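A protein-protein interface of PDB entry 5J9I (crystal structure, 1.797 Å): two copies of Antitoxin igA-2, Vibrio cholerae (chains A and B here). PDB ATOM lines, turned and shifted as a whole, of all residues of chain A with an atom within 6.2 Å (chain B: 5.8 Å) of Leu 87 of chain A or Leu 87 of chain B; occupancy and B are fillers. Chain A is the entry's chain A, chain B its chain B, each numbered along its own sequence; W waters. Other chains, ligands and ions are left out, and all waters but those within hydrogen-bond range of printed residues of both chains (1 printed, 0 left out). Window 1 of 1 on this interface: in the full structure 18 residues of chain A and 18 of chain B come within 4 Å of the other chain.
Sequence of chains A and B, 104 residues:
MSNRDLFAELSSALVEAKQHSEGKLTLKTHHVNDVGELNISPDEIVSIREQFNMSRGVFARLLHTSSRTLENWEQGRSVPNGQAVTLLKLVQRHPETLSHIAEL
The side-chain hydroxyl of Thr 65 of chain A lies within hydrogen-bond range of the side-chain amide nitrogen of Gln 83 of chain B (3.0 Å).
The backbone carbonyl oxygen (O) of Leu 63 of chain B sits at hydrogen-bond distance from the side-chain amide nitrogen (NE2) of Gln 83 of chain A (2.6 Å).
Of the printed residues of chain B, Leu 87 of chain A touches Leu 87 (3.9 Å).
Printed residues of chain B within 4 Å of Ile 101 of chain A: Thr 86 (3.9 Å) and Leu 90 (3.9 Å).
Printed residues of chain A within 4 Å of Gln 83 of chain B: Thr 65, Gln 83 and Ala 84.
Of the printed residues of chain A, Ala 84 of chain B touches Gln 83 (3.6 Å).
Leu 88 of chain A touches none of the printed residues of chain B.
Lys 89 of chain B touches none of the printed residues of chain A.
The nearest printed residue of chain B that does not touch Leu 87 of chain A is Leu 90 of chain B (4.01 Å).
The nearest residue of chain A that does not touch Leu 87 of chain B is Leu 90 of chain A (4.4 Å).
The nearest printed residue of chain A that does not touch Ile 101 of chain B is Leu 90 of chain A (4.4 Å).
O of Leu 63 of chain A sits at hydrogen-bond distance from OG1 of Thr 65 of chain A.
O of Gly 82 of chain A lies within hydrogen-bond range of OG1 of Thr 86 of chain A (2.9 Å).
O of Gly 82 of chain B sits at hydrogen-bond distance from OG1 of Thr 86 of chain B (3.2 Å).
Of the 14 printed residues of chain B, 8 touch a printed residue of chain A.
Printed residues of chain B that touch a printed residue of chain A: Leu 63, Gln 83, Ala 84, Thr 86, Leu 87, Leu 90, Thr 97 and Ile 101.
Hydrophobic or aromatic side chains of chain B within 4 Å of the printed part of chain A: Ala 84, Leu 87, Leu 90 and Ile 101.
Of the 15 printed residues of chain A, 8 touch a printed residue of chain B.
Printed residues of chain A that touch a printed residue of chain B: Thr 65, Gln 83, Ala 84, Thr 86, Leu 87, Leu 90, Thr 97 and Ile 101.
Hydrophobic or aromatic side chains of chain A within 4 Å of the printed part of chain B: Ala 84, Leu 87, Leu 90 and Ile 101.
Along chain A the printed residues that touch a printed residue of chain B span positions 65 to 101.
Among the printed residues, no Asp or Glu carboxylate lies within 4 Å of a Lys or Arg side-chain nitrogen of the other chain.
Water W1 lies within hydrogen-bond range of the backbone carbonyl oxygen of Leu 63 of chain A (2.6 Å), the side-chain hydroxyl of Thr 86 of chain B (2.7 Å) and the backbone carbonyl oxygen of Gly 82 of chain B (3.3 Å).
Gln 83 of chain A touches Ala 84 of chain B, and with the chains exchanged Ala 84 of chain A touches Gln 83 of chain B.
Thr 86 of chain A touches Leu 87 of chain B, but with the chains exchanged Leu 87 of chain A does not touch Thr 86 of chain B (4.1 Å).
Thr 86 of chain A touches Ile 101 of chain B, and with the chains exchanged Ile 101 of chain A touches Thr 86 of chain B.
Leu 87 of chain B touches its own counterpart, Leu 87 of chain A.
Of the 13 pairs that touch across the chains among the printed residues, 8 have their exchanged pair printed and touching as well.
Gln 83 of chain A touches Gln 83 of chain B.
CG of Gln 83 of chain A touches CB of Ala 84 of chain B, 3.6 Å away.
Gln 83 of chain A touches Leu 87 of chain B (O to CD1, 3.7 Å).
CB of Ala 84 of chain A touches CG of Gln 83 of chain B (3.5 Å).
CD1 of Leu 87 of chain B touches CG2 of Thr 86 of chain A, 3.7 Å away.
CD1 of Leu 87 of chain A touches CD2 of Leu 87 of chain B, 3.9 Å away.
Thr 97 of chain B touches Leu 90 of chain A.
CG2 of Thr 97 of chain A touches CD1 of Leu 90 of chain B, at 3.8 Å.
Ile 101 of chain A touches Thr 86 of chain B.
Leu 90 of chain B touches Ile 101 of chain A (CD2 to CG1, 3.9 Å).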
ATOM      1  N   LEU A  63       2.326 -20.656  18.468  1.00  0.00           N
ATOM      2  CA  LEU A  63       2.541 -19.880  19.721  1.00  0.00           C
ATOM      3  C   LEU A  63       2.585 -18.342  19.520  1.00  0.00           C
ATOM      4  O   LEU A  63       2.982 -17.586  20.415  1.00  0.00           O
ATOM      5  CB  LEU A  63       3.843 -20.346  20.392  1.00  0.00           C
ATOM      6  CG  LEU A  63       3.839 -21.739  21.017  1.00  0.00           C
ATOM      7  CD1 LEU A  63       5.212 -21.997  21.541  1.00  0.00           C
ATOM      8  CD2 LEU A  63       2.858 -21.816  22.142  1.00  0.00           C
ATOM      9  N   THR A  65       4.727 -16.652  18.007  1.00  0.00           N
ATOM     10  CA  THR A  65       6.099 -16.279  18.315  1.00  0.00           C
ATOM     11  C   THR A  65       6.814 -16.382  16.994  1.00  0.00           C
ATOM     12  O   THR A  65       6.438 -17.204  16.165  1.00  0.00           O
ATOM     13  CB  THR A  65       6.699 -17.231  19.384  1.00  0.00           C
ATOM     14  OG1 THR A  65       5.933 -17.179  20.613  1.00  0.00           O
ATOM     15  CG2 THR A  65       8.133 -16.943  19.661  1.00  0.00           C
ATOM     16  N   GLY A  82       9.390 -14.722  31.249  1.00  0.00           N
ATOM     17  CA  GLY A  82       8.603 -15.495  32.177  1.00  0.00           C
ATOM     18  C   GLY A  82       7.272 -15.927  31.603  1.00  0.00           C
ATOM     19  O   GLY A  82       6.830 -17.055  31.849  1.00  0.00           O
ATOM     20  N   GLN A  83       6.642 -15.077  30.787  1.00  0.00           N
ATOM     21  CA  GLN A  83       5.327 -15.473  30.220  1.00  0.00           C
ATOM     22  C   GLN A  83       5.481 -16.509  29.085  1.00  0.00           C
ATOM     23  O   GLN A  83       4.657 -17.400  28.942  1.00  0.00           O
ATOM     24  CB  GLN A  83       4.555 -14.252  29.712  1.00  0.00           C
ATOM     25  CG  GLN A  83       4.103 -13.308  30.862  1.00  0.00           C
ATOM     26  CD  GLN A  83       5.243 -12.468  31.381  1.00  0.00           C
ATOM     27  OE1 GLN A  83       6.053 -11.957  30.615  1.00  0.00           O
ATOM     28  NE2 GLN A  83       5.374 -12.414  32.705  1.00  0.00           N
ATOM     29  N   ALA A  84       6.570 -16.426  28.345  1.00  0.00           N
ATOM     30  CA  ALA A  84       6.846 -17.418  27.301  1.00  0.00           C
ATOM     31  C   ALA A  84       7.089 -18.769  27.944  1.00  0.00           C
ATOM     32  O   ALA A  84       6.588 -19.798  27.464  1.00  0.00           O
ATOM     33  CB  ALA A  84       8.051 -17.010  26.463  1.00  0.00           C
ATOM     34  N   VAL A  85       7.881 -18.776  29.027  1.00  0.00           N
ATOM     35  CA  VAL A  85       8.145 -20.021  29.740  1.00  0.00           C
ATOM     36  C   VAL A  85       6.816 -20.618  30.185  1.00  0.00           C
ATOM     37  O   VAL A  85       6.579 -21.800  29.999  1.00  0.00           O
ATOM     38  CB  VAL A  85       9.043 -19.816  30.969  1.00  0.00           C
ATOM     39  CG1 VAL A  85       9.070 -21.080  31.821  1.00  0.00           C
ATOM     40  CG2 VAL A  85      10.448 -19.439  30.555  1.00  0.00           C
ATOM     41  N   THR A  86       5.967 -19.788  30.769  1.00  0.00           N
ATOM     42  CA  THR A  86       4.635 -20.203  31.211  1.00  0.00           C
ATOM     43  C   THR A  86       3.859 -20.785  30.052  1.00  0.00           C
ATOM     44  O   THR A  86       3.297 -21.884  30.156  1.00  0.00           O
ATOM     45  CB  THR A  86       3.861 -19.014  31.833  1.00  0.00           C
ATOM     46  OG1 THR A  86       4.567 -18.543  32.986  1.00  0.00           O
ATOM     47  CG2 THR A  86       2.469 -19.406  32.234  1.00  0.00           C
ATOM     48  N   LEU A  87       3.831 -20.067  28.932  1.00  0.00           N
ATOM     49  CA  LEU A  87       3.173 -20.566  27.751  1.00  0.00           C
ATOM     50  C   LEU A  87       3.724 -21.898  27.246  1.00  0.00           C
ATOM     51  O   LEU A  87       2.983 -22.766  26.924  1.00  0.00           O
ATOM     52  CB  LEU A  87       3.308 -19.536  26.615  1.00  0.00           C
ATOM     53  CG  LEU A  87       2.445 -19.687  25.387  1.00  0.00           C
ATOM     54  CD1 LEU A  87       1.000 -19.760  25.767  1.00  0.00           C
ATOM     55  CD2 LEU A  87       2.756 -18.442  24.503  1.00  0.00           C
ATOM     56  N   LEU A  88       5.036 -22.049  27.171  1.00  0.00           N
ATOM     57  CA  LEU A  88       5.582 -23.319  26.688  1.00  0.00           C
ATOM     58  C   LEU A  88       5.190 -24.450  27.623  1.00  0.00           C
ATOM     59  O   LEU A  88       4.795 -25.555  27.228  1.00  0.00           O
ATOM     60  CB  LEU A  88       7.119 -23.243  26.597  1.00  0.00           C
ATOM     61  CG  LEU A  88       7.579 -22.289  25.504  1.00  0.00           C
ATOM     62  CD1 LEU A  88       9.027 -21.810  25.775  1.00  0.00           C
ATOM     63  CD2 LEU A  88       7.503 -22.994  24.139  1.00  0.00           C
ATOM     64  N   LYS A  89       5.286 -24.180  28.916  1.00  0.00           N
ATOM     65  CA  LYS A  89       5.003 -25.231  29.870  1.00  0.00           C
ATOM     66  C   LYS A  89       3.526 -25.615  29.812  1.00  0.00           C
ATOM     67  O   LYS A  89       3.171 -26.768  30.000  1.00  0.00           O
ATOM     68  CB  LYS A  89       5.365 -24.813  31.304  1.00  0.00           C
ATOM     69  CG  LYS A  89       6.880 -24.671  31.530  1.00  0.00           C
ATOM     70  CD  LYS A  89       7.288 -24.409  33.014  1.00  0.00           C
ATOM     71  CE  LYS A  89       7.180 -25.729  33.807  1.00  0.00           C
ATOM     72  NZ  LYS A  89       8.047 -26.866  33.278  1.00  0.00           N
ATOM     73  N   LEU A  90       2.681 -24.631  29.562  1.00  0.00           N
ATOM     74  CA  LEU A  90       1.248 -24.875  29.440  1.00  0.00           C
ATOM     75  C   LEU A  90       0.920 -25.814  28.287  1.00  0.00           C
ATOM     76  O   LEU A  90       0.094 -26.715  28.378  1.00  0.00           O
ATOM     77  CB  LEU A  90       0.544 -23.557  29.239  1.00  0.00           C
ATOM     78  CG  LEU A  90      -0.987 -23.532  29.195  1.00  0.00           C
ATOM     79  CD1 LEU A  90      -1.586 -24.000  30.488  1.00  0.00           C
ATOM     80  CD2 LEU A  90      -1.509 -22.120  28.910  1.00  0.00           C
ATOM     81  N   VAL A  91       1.538 -25.537  27.158  1.00  0.00           N
ATOM     82  CA  VAL A  91       1.300 -26.302  25.945  1.00  0.00           C
ATOM     83  C   VAL A  91       1.783 -27.727  26.112  1.00  0.00           C
ATOM     84  O   VAL A  91       1.174 -28.683  25.608  1.00  0.00           O
ATOM     85  CB  VAL A  91       1.997 -25.578  24.792  1.00  0.00           C
ATOM     86  CG1 VAL A  91       2.188 -26.461  23.613  1.00  0.00           C
ATOM     87  CG2 VAL A  91       1.119 -24.361  24.437  1.00  0.00           C
ATOM     88  N   GLN A  92       2.894 -27.855  26.836  1.00  0.00           N
ATOM     89  CA  GLN A  92       3.520 -29.131  27.073  1.00  0.00           C
ATOM     90  C   GLN A  92       2.538 -30.076  27.744  1.00  0.00           C
ATOM     91  O   GLN A  92       2.350 -31.220  27.309  1.00  0.00           O
ATOM     92  CB  GLN A  92       4.750 -28.958  27.982  1.00  0.00           C
ATOM     93  CG  GLN A  92       5.573 -30.200  28.185  1.00  0.00           C
ATOM     94  CD  GLN A  92       6.709 -29.990  29.176  1.00  0.00           C
ATOM     95  OE1 GLN A  92       6.663 -29.098  30.038  1.00  0.00           O
ATOM     96  NE2 GLN A  92       7.770 -30.769  29.011  1.00  0.00           N
ATOM     97  N   THR A  97      -4.174 -26.477  24.351  1.00  0.00           N
ATOM     98  CA  THR A  97      -3.936 -25.030  24.367  1.00  0.00           C
ATOM     99  C   THR A  97      -3.582 -24.471  22.962  1.00  0.00           C
ATOM    100  O   THR A  97      -3.886 -23.323  22.658  1.00  0.00           O
ATOM    101  CB  THR A  97      -2.788 -24.637  25.339  1.00  0.00           C
ATOM    102  OG1 THR A  97      -3.009 -25.220  26.609  1.00  0.00           O
ATOM    103  CG2 THR A  97      -2.678 -23.108  25.489  1.00  0.00           C
ATOM    104  N   ILE A 101      -5.425 -21.291  21.219  1.00  0.00           N
ATOM    105  CA  ILE A 101      -4.753 -20.125  20.733  1.00  0.00           C
ATOM    106  C   ILE A 101      -5.166 -19.792  19.325  1.00  0.00           C
ATOM    107  O   ILE A 101      -5.312 -18.629  18.960  1.00  0.00           O
ATOM    108  CB  ILE A 101      -3.252 -20.308  20.762  1.00  0.00           C
ATOM    109  CG1 ILE A 101      -2.752 -20.270  22.222  1.00  0.00           C
ATOM    110  CG2 ILE A 101      -2.554 -19.200  20.004  1.00  0.00           C
ATOM    111  CD1 ILE A 101      -1.315 -20.691  22.370  1.00  0.00           C
ATOM    112  N   LEU B  63       1.364 -15.296  36.306  1.00  0.00           N
ATOM    113  CA  LEU B  63       1.770 -14.793  34.998  1.00  0.00           C
ATOM    114  C   LEU B  63       3.271 -14.559  34.984  1.00  0.00           C
ATOM    115  O   LEU B  63       3.812 -14.023  34.028  1.00  0.00           O
ATOM    116  CB  LEU B  63       1.052 -13.504  34.656  1.00  0.00           C
ATOM    117  CG  LEU B  63      -0.457 -13.492  34.456  1.00  0.00           C
ATOM    118  CD1 LEU B  63      -1.022 -12.114  34.266  1.00  0.00           C
ATOM    119  CD2 LEU B  63      -0.772 -14.414  33.272  1.00  0.00           C
ATOM    120  N   GLY B  82       4.523 -10.148  23.711  1.00  0.00           N
ATOM    121  CA  GLY B  82       3.618 -11.026  22.948  1.00  0.00           C
ATOM    122  C   GLY B  82       3.150 -12.294  23.625  1.00  0.00           C
ATOM    123  O   GLY B  82       1.972 -12.649  23.539  1.00  0.00           O
ATOM    124  N   GLN B  83       4.034 -12.982  24.354  1.00  0.00           N
ATOM    125  CA  GLN B  83       3.614 -14.165  25.052  1.00  0.00           C
ATOM    126  C   GLN B  83       2.698 -13.815  26.216  1.00  0.00           C
ATOM    127  O   GLN B  83       1.733 -14.535  26.458  1.00  0.00           O
ATOM    128  CB  GLN B  83       4.817 -14.968  25.531  1.00  0.00           C
ATOM    129  CG  GLN B  83       5.610 -15.618  24.384  1.00  0.00           C
ATOM    130  CD  GLN B  83       6.477 -14.627  23.662  1.00  0.00           C
ATOM    131  OE1 GLN B  83       6.953 -13.642  24.254  1.00  0.00           O
ATOM    132  NE2 GLN B  83       6.744 -14.884  22.384  1.00  0.00           N
ATOM    133  N   ALA B  84       2.919 -12.651  26.833  1.00  0.00           N
ATOM    134  CA  ALA B  84       2.055 -12.199  27.906  1.00  0.00           C
ATOM    135  C   ALA B  84       0.637 -11.934  27.380  1.00  0.00           C
ATOM    136  O   ALA B  84      -0.322 -12.361  27.990  1.00  0.00           O
ATOM    137  CB  ALA B  84       2.618 -10.945  28.563  1.00  0.00           C
ATOM    138  N   VAL B  85       0.543 -11.294  26.214  1.00  0.00           N
ATOM    139  CA  VAL B  85      -0.755 -11.040  25.593  1.00  0.00           C
ATOM    140  C   VAL B  85      -1.489 -12.333  25.289  1.00  0.00           C
ATOM    141  O   VAL B  85      -2.709 -12.454  25.506  1.00  0.00           O
ATOM    142  CB  VAL B  85      -0.614 -10.197  24.287  1.00  0.00           C
ATOM    143  CG1 VAL B  85      -1.916 -10.121  23.563  1.00  0.00           C
ATOM    144  CG2 VAL B  85      -0.150  -8.793  24.627  1.00  0.00           C
ATOM    145  N   THR B  86      -0.765 -13.291  24.728  1.00  0.00           N
ATOM    146  CA  THR B  86      -1.340 -14.601  24.465  1.00  0.00           C
ATOM    147  C   THR B  86      -1.875 -15.272  25.709  1.00  0.00           C
ATOM    148  O   THR B  86      -2.954 -15.850  25.711  1.00  0.00           O
ATOM    149  CB  THR B  86      -0.286 -15.551  23.786  1.00  0.00           C
ATOM    150  OG1 THR B  86       0.120 -14.990  22.530  1.00  0.00           O
ATOM    151  CG2 THR B  86      -0.888 -16.951  23.522  1.00  0.00           C
ATOM    152  N   LEU B  87      -1.098 -15.238  26.788  1.00  0.00           N
ATOM    153  CA  LEU B  87      -1.563 -15.791  28.051  1.00  0.00           C
ATOM    154  C   LEU B  87      -2.788 -15.096  28.560  1.00  0.00           C
ATOM    155  O   LEU B  87      -3.715 -15.740  28.981  1.00  0.00           O
ATOM    156  CB  LEU B  87      -0.496 -15.692  29.146  1.00  0.00           C
ATOM    157  CG  LEU B  87       0.664 -16.660  29.226  1.00  0.00           C
ATOM    158  CD1 LEU B  87       1.487 -16.309  30.470  1.00  0.00           C
ATOM    159  CD2 LEU B  87       0.228 -18.126  29.263  1.00  0.00           C
ATOM    160  N   LEU B  88      -2.798 -13.769  28.472  1.00  0.00           N
ATOM    161  CA  LEU B  88      -3.942 -13.011  28.925  1.00  0.00           C
ATOM    162  C   LEU B  88      -5.202 -13.371  28.119  1.00  0.00           C
ATOM    163  O   LEU B  88      -6.273 -13.575  28.690  1.00  0.00           O
ATOM    164  CB  LEU B  88      -3.639 -11.508  28.851  1.00  0.00           C
ATOM    165  CG  LEU B  88      -2.644 -11.013  29.930  1.00  0.00           C
ATOM    166  CD1 LEU B  88      -1.993  -9.730  29.573  1.00  0.00           C
ATOM    167  CD2 LEU B  88      -3.414 -10.863  31.193  1.00  0.00           C
ATOM    168  N   LYS B  89      -5.110 -13.443  26.798  1.00  0.00           N
ATOM    169  CA  LYS B  89      -6.315 -13.753  26.013  1.00  0.00           C
ATOM    170  C   LYS B  89      -6.801 -15.180  26.230  1.00  0.00           C
ATOM    171  O   LYS B  89      -8.002 -15.491  26.131  1.00  0.00           O
ATOM    172  CB  LYS B  89      -6.052 -13.515  24.520  1.00  0.00           C
ATOM    173  CG  LYS B  89      -5.802 -12.060  24.216  1.00  0.00           C
ATOM    174  CD  LYS B  89      -5.650 -11.799  22.713  1.00  0.00           C
ATOM    175  CE  LYS B  89      -6.992 -11.825  21.985  1.00  0.00           C
ATOM    176  NZ  LYS B  89      -7.902 -10.766  22.517  1.00  0.00           N
ATOM    177  N   LEU B  90      -5.875 -16.097  26.466  1.00  0.00           N
ATOM    178  CA  LEU B  90      -6.252 -17.451  26.872  1.00  0.00           C
ATOM    179  C   LEU B  90      -7.047 -17.503  28.171  1.00  0.00           C
ATOM    180  O   LEU B  90      -8.125 -18.087  28.236  1.00  0.00           O
ATOM    181  CB  LEU B  90      -4.997 -18.298  27.019  1.00  0.00           C
ATOM    182  CG  LEU B  90      -4.345 -18.934  25.820  1.00  0.00           C
ATOM    183  CD1 LEU B  90      -2.966 -19.428  26.237  1.00  0.00           C
ATOM    184  CD2 LEU B  90      -5.220 -20.092  25.286  1.00  0.00           C
ATOM    185  N   VAL B  91      -6.552 -16.801  29.182  1.00  0.00           N
ATOM    186  CA  VAL B  91      -7.171 -16.798  30.501  1.00  0.00           C
ATOM    187  C   VAL B  91      -8.511 -16.074  30.359  1.00  0.00           C
ATOM    188  O   VAL B  91      -9.486 -16.396  31.026  1.00  0.00           O
ATOM    189  CB  VAL B  91      -6.205 -16.154  31.490  1.00  0.00           C
ATOM    190  CG1 VAL B  91      -6.906 -15.627  32.662  1.00  0.00           C
ATOM    191  CG2 VAL B  91      -5.149 -17.206  31.874  1.00  0.00           C
ATOM    192  N   GLN B  92      -8.532 -15.078  29.494  1.00  0.00           N
ATOM    193  CA  GLN B  92      -9.764 -14.350  29.229  1.00  0.00           C
ATOM    194  C   GLN B  92     -10.855 -15.226  28.652  1.00  0.00           C
ATOM    195  O   GLN B  92     -12.011 -15.154  29.080  1.00  0.00           O
ATOM    196  CB  GLN B  92      -9.509 -13.185  28.254  1.00  0.00           C
ATOM    197  CG  GLN B  92     -10.757 -12.371  27.893  1.00  0.00           C
ATOM    198  CD  GLN B  92     -10.461 -11.257  26.908  1.00  0.00           C
ATOM    199  OE1 GLN B  92      -9.848 -11.475  25.854  1.00  0.00           O
ATOM    200  NE2 GLN B  92     -10.886 -10.053  27.247  1.00  0.00           N
ATOM    201  N   THR B  97      -7.818 -22.032  32.331  1.00  0.00           N
ATOM    202  CA  THR B  97      -6.392 -21.904  32.056  1.00  0.00           C
ATOM    203  C   THR B  97      -5.589 -21.413  33.233  1.00  0.00           C
ATOM    204  O   THR B  97      -4.421 -21.759  33.374  1.00  0.00           O
ATOM    205  CB  THR B  97      -6.130 -20.935  30.882  1.00  0.00           C
ATOM    206  OG1 THR B  97      -6.855 -21.370  29.732  1.00  0.00           O
ATOM    207  CG2 THR B  97      -4.643 -20.870  30.532  1.00  0.00           C
ATOM    208  N   ILE B 101      -2.208 -22.984  34.880  1.00  0.00           N
ATOM    209  CA  ILE B 101      -1.013 -22.197  35.027  1.00  0.00           C
ATOM    210  C   ILE B 101      -0.498 -22.298  36.449  1.00  0.00           C
ATOM    211  O   ILE B 101       0.706 -22.374  36.683  1.00  0.00           O
ATOM    212  CB  ILE B 101      -1.275 -20.718  34.681  1.00  0.00           C
ATOM    213  CG1 ILE B 101      -1.370 -20.556  33.171  1.00  0.00           C
ATOM    214  CG2 ILE B 101      -0.145 -19.853  35.179  1.00  0.00           C
ATOM    215  CD1 ILE B 101      -1.898 -19.173  32.715  1.00  0.00           C
HETATM  216  O   HOH W   1       2.741 -15.541  22.083  1.00  0.00           O
